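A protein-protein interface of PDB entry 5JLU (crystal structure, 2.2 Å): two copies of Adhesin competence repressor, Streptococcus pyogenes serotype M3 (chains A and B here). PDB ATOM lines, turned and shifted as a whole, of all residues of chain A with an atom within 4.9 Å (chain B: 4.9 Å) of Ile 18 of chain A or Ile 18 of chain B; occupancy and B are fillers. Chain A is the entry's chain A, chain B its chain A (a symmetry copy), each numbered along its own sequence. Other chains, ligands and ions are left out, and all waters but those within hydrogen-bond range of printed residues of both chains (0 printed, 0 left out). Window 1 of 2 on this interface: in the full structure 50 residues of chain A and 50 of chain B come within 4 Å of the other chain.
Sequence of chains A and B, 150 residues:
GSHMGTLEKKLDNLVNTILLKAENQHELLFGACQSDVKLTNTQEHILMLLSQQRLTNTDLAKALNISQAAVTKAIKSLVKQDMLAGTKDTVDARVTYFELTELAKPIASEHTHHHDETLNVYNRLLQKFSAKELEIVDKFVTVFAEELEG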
ATOM      1  N   LEU A  14      16.060   7.140  -7.632  1.00  0.00           N
ATOM      2  CA  LEU A  14      17.134   7.447  -6.700  1.00  0.00           C
ATOM      3  C   LEU A  14      16.534   7.760  -5.350  1.00  0.00           C
ATOM      4  O   LEU A  14      16.925   7.202  -4.360  1.00  0.00           O
ATOM      5  CB  LEU A  14      17.998   8.576  -7.218  1.00  0.00           C
ATOM      6  CG  LEU A  14      19.174   8.998  -6.341  1.00  0.00           C
ATOM      7  CD1 LEU A  14      20.190   7.882  -6.148  1.00  0.00           C
ATOM      8  CD2 LEU A  14      19.820  10.187  -7.012  1.00  0.00           C
ATOM      9  N   VAL A  15      15.532   8.622  -5.310  1.00  0.00           N
ATOM     10  CA  VAL A  15      14.874   8.905  -4.058  1.00  0.00           C
ATOM     11  C   VAL A  15      14.295   7.622  -3.358  1.00  0.00           C
ATOM     12  O   VAL A  15      14.375   7.455  -2.101  1.00  0.00           O
ATOM     13  CB  VAL A  15      13.847  10.022  -4.298  1.00  0.00           C
ATOM     14  CG1 VAL A  15      12.978  10.314  -3.088  1.00  0.00           C
ATOM     15  CG2 VAL A  15      14.555  11.296  -4.706  1.00  0.00           C
ATOM     16  N   ASN A  16      13.730   6.713  -4.167  1.00  0.00           N
ATOM     17  CA  ASN A  16      13.096   5.523  -3.629  1.00  0.00           C
ATOM     18  C   ASN A  16      14.103   4.598  -3.051  1.00  0.00           C
ATOM     19  O   ASN A  16      13.804   3.995  -1.984  1.00  0.00           O
ATOM     20  CB  ASN A  16      12.235   4.751  -4.696  1.00  0.00           C
ATOM     21  CG  ASN A  16      10.979   5.523  -5.084  1.00  0.00           C
ATOM     22  OD1 ASN A  16      10.539   6.458  -4.370  1.00  0.00           O
ATOM     23  ND2 ASN A  16      10.422   5.186  -6.204  1.00  0.00           N
ATOM     24  N   THR A  17      15.255   4.468  -3.727  1.00  0.00           N
ATOM     25  CA  THR A  17      16.292   3.571  -3.235  1.00  0.00           C
ATOM     26  C   THR A  17      16.882   4.133  -1.951  1.00  0.00           C
ATOM     27  O   THR A  17      17.076   3.370  -0.973  1.00  0.00           O
ATOM     28  CB  THR A  17      17.380   3.104  -4.271  1.00  0.00           C
ATOM     29  OG1 THR A  17      18.614   3.743  -4.026  1.00  0.00           O
ATOM     30  CG2 THR A  17      16.978   3.237  -5.631  1.00  0.00           C
ATOM     31  N   ILE A  18      16.999   5.443  -1.842  1.00  0.00           N
ATOM     32  CA  ILE A  18      17.389   6.023  -0.517  1.00  0.00           C
ATOM     33  C   ILE A  18      16.366   5.689   0.540  1.00  0.00           C
ATOM     34  O   ILE A  18      16.718   5.263   1.618  1.00  0.00           O
ATOM     35  CB  ILE A  18      17.636   7.532  -0.568  1.00  0.00           C
ATOM     36  CG1 ILE A  18      18.942   7.816  -1.338  1.00  0.00           C
ATOM     37  CG2 ILE A  18      17.698   8.174   0.834  1.00  0.00           C
ATOM     38  CD1 ILE A  18      18.962   9.206  -1.903  1.00  0.00           C
ATOM     39  N   LEU A  19      15.096   5.898   0.254  1.00  0.00           N
ATOM     40  CA  LEU A  19      14.072   5.586   1.261  1.00  0.00           C
ATOM     41  C   LEU A  19      14.063   4.067   1.604  1.00  0.00           C
ATOM     42  O   LEU A  19      14.082   3.688   2.803  1.00  0.00           O
ATOM     43  CB  LEU A  19      12.706   6.120   0.831  1.00  0.00           C
ATOM     44  CG  LEU A  19      12.576   7.661   0.651  1.00  0.00           C
ATOM     45  CD1 LEU A  19      11.210   8.094   0.154  1.00  0.00           C
ATOM     46  CD2 LEU A  19      12.842   8.348   1.986  1.00  0.00           C
ATOM     47  N   LEU A  20      14.118   3.208   0.585  1.00  0.00           N
ATOM     48  CA  LEU A  20      14.044   1.766   0.812  1.00  0.00           C
ATOM     49  C   LEU A  20      15.223   1.154   1.544  1.00  0.00           C
ATOM     50  O   LEU A  20      15.065   0.162   2.310  1.00  0.00           O
ATOM     51  CB  LEU A  20      13.867   0.998  -0.474  1.00  0.00           C
ATOM     52  CG  LEU A  20      12.589   1.380  -1.231  1.00  0.00           C
ATOM     53  CD1 LEU A  20      12.657   0.698  -2.609  1.00  0.00           C
ATOM     54  CD2 LEU A  20      11.337   1.040  -0.493  1.00  0.00           C
ATOM     55  N   LYS A  21      16.412   1.655   1.234  1.00  0.00           N
ATOM     56  CA  LYS A  21      17.625   1.234   1.927  1.00  0.00           C
ATOM     57  C   LYS A  21      17.606   1.624   3.389  1.00  0.00           C
ATOM     58  O   LYS A  21      17.905   0.808   4.208  1.00  0.00           O
ATOM     59  CB  LYS A  21      18.850   1.871   1.277  1.00  0.00           C
ATOM     60  CG  LYS A  21      19.186   1.217  -0.023  1.00  0.00           C
ATOM     61  CD  LYS A  21      19.990  -0.092   0.199  1.00  0.00           C
ATOM     62  CE  LYS A  21      19.835  -1.070  -0.968  1.00  0.00           C
ATOM     63  NZ  LYS A  21      18.475  -1.677  -1.033  1.00  0.00           N
ATOM     64  N   ALA A  22      17.238   2.870   3.696  1.00  0.00           N
ATOM     65  CA  ALA A  22      17.114   3.302   5.066  1.00  0.00           C
ATOM     66  C   ALA A  22      16.080   2.476   5.875  1.00  0.00           C
ATOM     67  O   ALA A  22      16.283   2.233   7.054  1.00  0.00           O
ATOM     68  CB  ALA A  22      16.763   4.762   5.105  1.00  0.00           C
ATOM     69  N   LEU A 148      13.987  19.857  -3.028  1.00  0.00           N
ATOM     70  CA  LEU A 148      13.606  18.882  -1.958  1.00  0.00           C
ATOM     71  C   LEU A 148      13.394  19.463  -0.563  1.00  0.00           C
ATOM     72  O   LEU A 148      12.659  18.865   0.230  1.00  0.00           O
ATOM     73  CB  LEU A 148      14.632  17.768  -1.819  1.00  0.00           C
ATOM     74  CG  LEU A 148      14.492  16.686  -2.876  1.00  0.00           C
ATOM     75  CD1 LEU A 148      15.660  15.734  -2.679  1.00  0.00           C
ATOM     76  CD2 LEU A 148      13.146  15.948  -2.870  1.00  0.00           C
ATOM     77  N   LEU B  14      22.174  15.992   1.077  1.00  0.00           N
ATOM     78  CA  LEU B  14      21.077  15.667   0.180  1.00  0.00           C
ATOM     79  C   LEU B  14      20.387  14.421   0.683  1.00  0.00           C
ATOM     80  O   LEU B  14      19.196  14.402   0.843  1.00  0.00           O
ATOM     81  CB  LEU B  14      21.565  15.515  -1.244  1.00  0.00           C
ATOM     82  CG  LEU B  14      20.512  15.182  -2.298  1.00  0.00           C
ATOM     83  CD1 LEU B  14      19.458  16.271  -2.437  1.00  0.00           C
ATOM     84  CD2 LEU B  14      21.243  14.989  -3.605  1.00  0.00           C
ATOM     85  N   VAL B  15      21.145  13.383   0.993  1.00  0.00           N
ATOM     86  CA  VAL B  15      20.547  12.193   1.545  1.00  0.00           C
ATOM     87  C   VAL B  15      19.725  12.464   2.858  1.00  0.00           C
ATOM     88  O   VAL B  15      18.615  11.887   3.080  1.00  0.00           O
ATOM     89  CB  VAL B  15      21.643  11.126   1.685  1.00  0.00           C
ATOM     90  CG1 VAL B  15      21.176   9.869   2.395  1.00  0.00           C
ATOM     91  CG2 VAL B  15      22.171  10.745   0.319  1.00  0.00           C
ATOM     92  N   ASN B  16      20.256  13.348   3.715  1.00  0.00           N
ATOM     93  CA  ASN B  16      19.626  13.624   4.993  1.00  0.00           C
ATOM     94  C   ASN B  16      18.345  14.352   4.809  1.00  0.00           C
ATOM     95  O   ASN B  16      17.379  14.041   5.559  1.00  0.00           O
ATOM     96  CB  ASN B  16      20.550  14.442   5.968  1.00  0.00           C
ATOM     97  CG  ASN B  16      21.728  13.614   6.469  1.00  0.00           C
ATOM     98  OD1 ASN B  16      21.728  12.361   6.388  1.00  0.00           O
ATOM     99  ND2 ASN B  16      22.735  14.277   6.942  1.00  0.00           N
ATOM    100  N   THR B  17      18.324  15.300   3.859  1.00  0.00           N
ATOM    101  CA  THR B  17      17.111  16.068   3.622  1.00  0.00           C
ATOM    102  C   THR B  17      16.047  15.164   3.017  1.00  0.00           C
ATOM    103  O   THR B  17      14.870  15.217   3.451  1.00  0.00           O
ATOM    104  CB  THR B  17      17.270  17.438   2.864  1.00  0.00           C
ATOM    105  OG1 THR B  17      16.787  17.340   1.542  1.00  0.00           O
ATOM    106  CG2 THR B  17      18.591  17.969   2.904  1.00  0.00           C
ATOM    107  N   ILE B  18      16.435  14.220   2.182  1.00  0.00           N
ATOM    108  CA  ILE B  18      15.436  13.199   1.734  1.00  0.00           C
ATOM    109  C   ILE B  18      14.907  12.411   2.906  1.00  0.00           C
ATOM    110  O   ILE B  18      13.715  12.231   3.033  1.00  0.00           O
ATOM    111  CB  ILE B  18      15.976  12.258   0.654  1.00  0.00           C
ATOM    112  CG1 ILE B  18      16.130  13.030  -0.673  1.00  0.00           C
ATOM    113  CG2 ILE B  18      15.083  11.017   0.445  1.00  0.00           C
ATOM    114  CD1 ILE B  18      17.134  12.380  -1.579  1.00  0.00           C
ATOM    115  N   LEU B  19      15.781  11.916   3.759  1.00  0.00           N
ATOM    116  CA  LEU B  19      15.302  11.142   4.912  1.00  0.00           C
ATOM    117  C   LEU B  19      14.418  12.016   5.851  1.00  0.00           C
ATOM    118  O   LEU B  19      13.297  11.599   6.236  1.00  0.00           O
ATOM    119  CB  LEU B  19      16.465  10.462   5.633  1.00  0.00           C
ATOM    120  CG  LEU B  19      17.289   9.422   4.817  1.00  0.00           C
ATOM    121  CD1 LEU B  19      18.465   8.852   5.586  1.00  0.00           C
ATOM    122  CD2 LEU B  19      16.378   8.269   4.408  1.00  0.00           C
ATOM    123  N   LEU B  20      14.865  13.238   6.151  1.00  0.00           N
ATOM    124  CA  LEU B  20      14.135  14.098   7.079  1.00  0.00           C
ATOM    125  C   LEU B  20      12.779  14.583   6.599  1.00  0.00           C
ATOM    126  O   LEU B  20      11.836  14.779   7.415  1.00  0.00           O
ATOM    127  CB  LEU B  20      14.933  15.315   7.471  1.00  0.00           C
ATOM    128  CG  LEU B  20      16.259  14.968   8.160  1.00  0.00           C
ATOM    129  CD1 LEU B  20      17.058  16.276   8.293  1.00  0.00           C
ATOM    130  CD2 LEU B  20      16.084  14.277   9.471  1.00  0.00           C
ATOM    131  N   LYS B  21      12.704  14.887   5.310  1.00  0.00           N
ATOM    132  CA  LYS B  21      11.443  15.273   4.686  1.00  0.00           C
ATOM    133  C   LYS B  21      10.437  14.143   4.696  1.00  0.00           C
ATOM    134  O   LYS B  21       9.320  14.367   5.052  1.00  0.00           O
ATOM    135  CB  LYS B  21      11.679  15.692   3.238  1.00  0.00           C
ATOM    136  CG  LYS B  21      12.308  17.044   3.151  1.00  0.00           C
ATOM    137  CD  LYS B  21      11.247  18.167   3.298  1.00  0.00           C
ATOM    138  CE  LYS B  21      11.856  19.473   3.813  1.00  0.00           C
ATOM    139  NZ  LYS B  21      12.265  19.393   5.244  1.00  0.00           N
ATOM    140  N   ALA B  22      10.856  12.933   4.316  1.00  0.00           N
ATOM    141  CA  ALA B  22       9.987  11.783   4.372  1.00  0.00           C
ATOM    142  C   ALA B  22       9.464  11.484   5.800  1.00  0.00           C
ATOM    143  O   ALA B  22       8.331  11.056   5.957  1.00  0.00           O
ATOM    144  CB  ALA B  22      10.700  10.585   3.814  1.00  0.00           C
ATOM    145  N   LEU B 148      24.528   3.478  -3.930  1.00  0.00           N
ATOM    146  CA  LEU B 148      23.447   3.395  -2.899  1.00  0.00           C
ATOM    147  C   LEU B 148      22.657   2.091  -2.855  1.00  0.00           C
ATOM    148  O   LEU B 148      22.105   1.759  -1.800  1.00  0.00           O
ATOM    149  CB  LEU B 148      22.433   4.518  -3.055  1.00  0.00           C
ATOM    150  CG  LEU B 148      22.905   5.840  -2.476  1.00  0.00           C
ATOM    151  CD1 LEU B 148      21.847   6.872  -2.830  1.00  0.00           C
ATOM    152  CD2 LEU B 148      23.198   5.818  -0.969  1.00  0.00           C
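Leu 148 of chain B touches Leu 14 of chain A (CD1 to CD1, 3.8 Å).
CD1 of Ile 18 of chain B touches CD1 of Ile 18 of chain A, at 3.7 Å.
Leu 19 of chain B touches Ile 18 of chain A (CD2 to CG2, 3.8 Å).
Ile 18 of chain A touches Leu 148 of chain B.
Leu 19 of chain A touches Ile 18 of chain B.
Ala 22 of chain B touches Leu 19 of chain A (CB to CD2, 3.6 Å).
CD2 of Leu 19 of chain B touches CB of Ala 22 of chain A (3.6 Å).
Leu 14 of chain B touches Leu 148 of chain A.
Leu 148 of chain A touches Ile 18 of chain B.
Leu 148 of chain A touches Lys 21 of chain B.
Printed residues of chain B within 4 Å of Leu 19 of chain A: Ile 18 (3.8 Å) and Ala 22 (3.6 Å).
Of the printed residues of chain B, Leu 148 of chain A touches Leu 14, Ile 18 and Lys 21.
Of the printed residues of chain A, Leu 14 of chain B touches Leu 148.
Of chain A, only Ile 18, Leu 19 and Leu 148 come within 4 Å of Ile 18 of chain B.
Of the printed residues of chain A, Lys 21 of chain B touches Leu 148.
The nearest printed residue of chain B that does not touch Leu 19 of chain A is Leu 19 of chain B (4.3 Å).
Of the 10 printed residues of chain B, 6 touch a printed residue of chain A.
Along chain B the printed residues that touch a printed residue of chain A span positions 14 to 148.
Among the printed residues, 11 pairs touch across the chains.
Leu 14 of chain A touches Leu 148 of chain B, and with the chains exchanged Leu 148 of chain A touches Leu 14 of chain B.
Ile 18 of chain B touches its own counterpart, Ile 18 of chain A.
Leu 19 of chain A touches Ala 22 of chain B, and with the chains exchanged Ala 22 of chain A touches Leu 19 of chain B.
Lys 21 of chain A touches Leu 148 of chain B, and with the chains exchanged Leu 148 of chain A touches Lys 21 of chain B.
Positions printed for both chains: 14, 15, 16, 17, 18, 19, 20, 21, 22 and 148.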
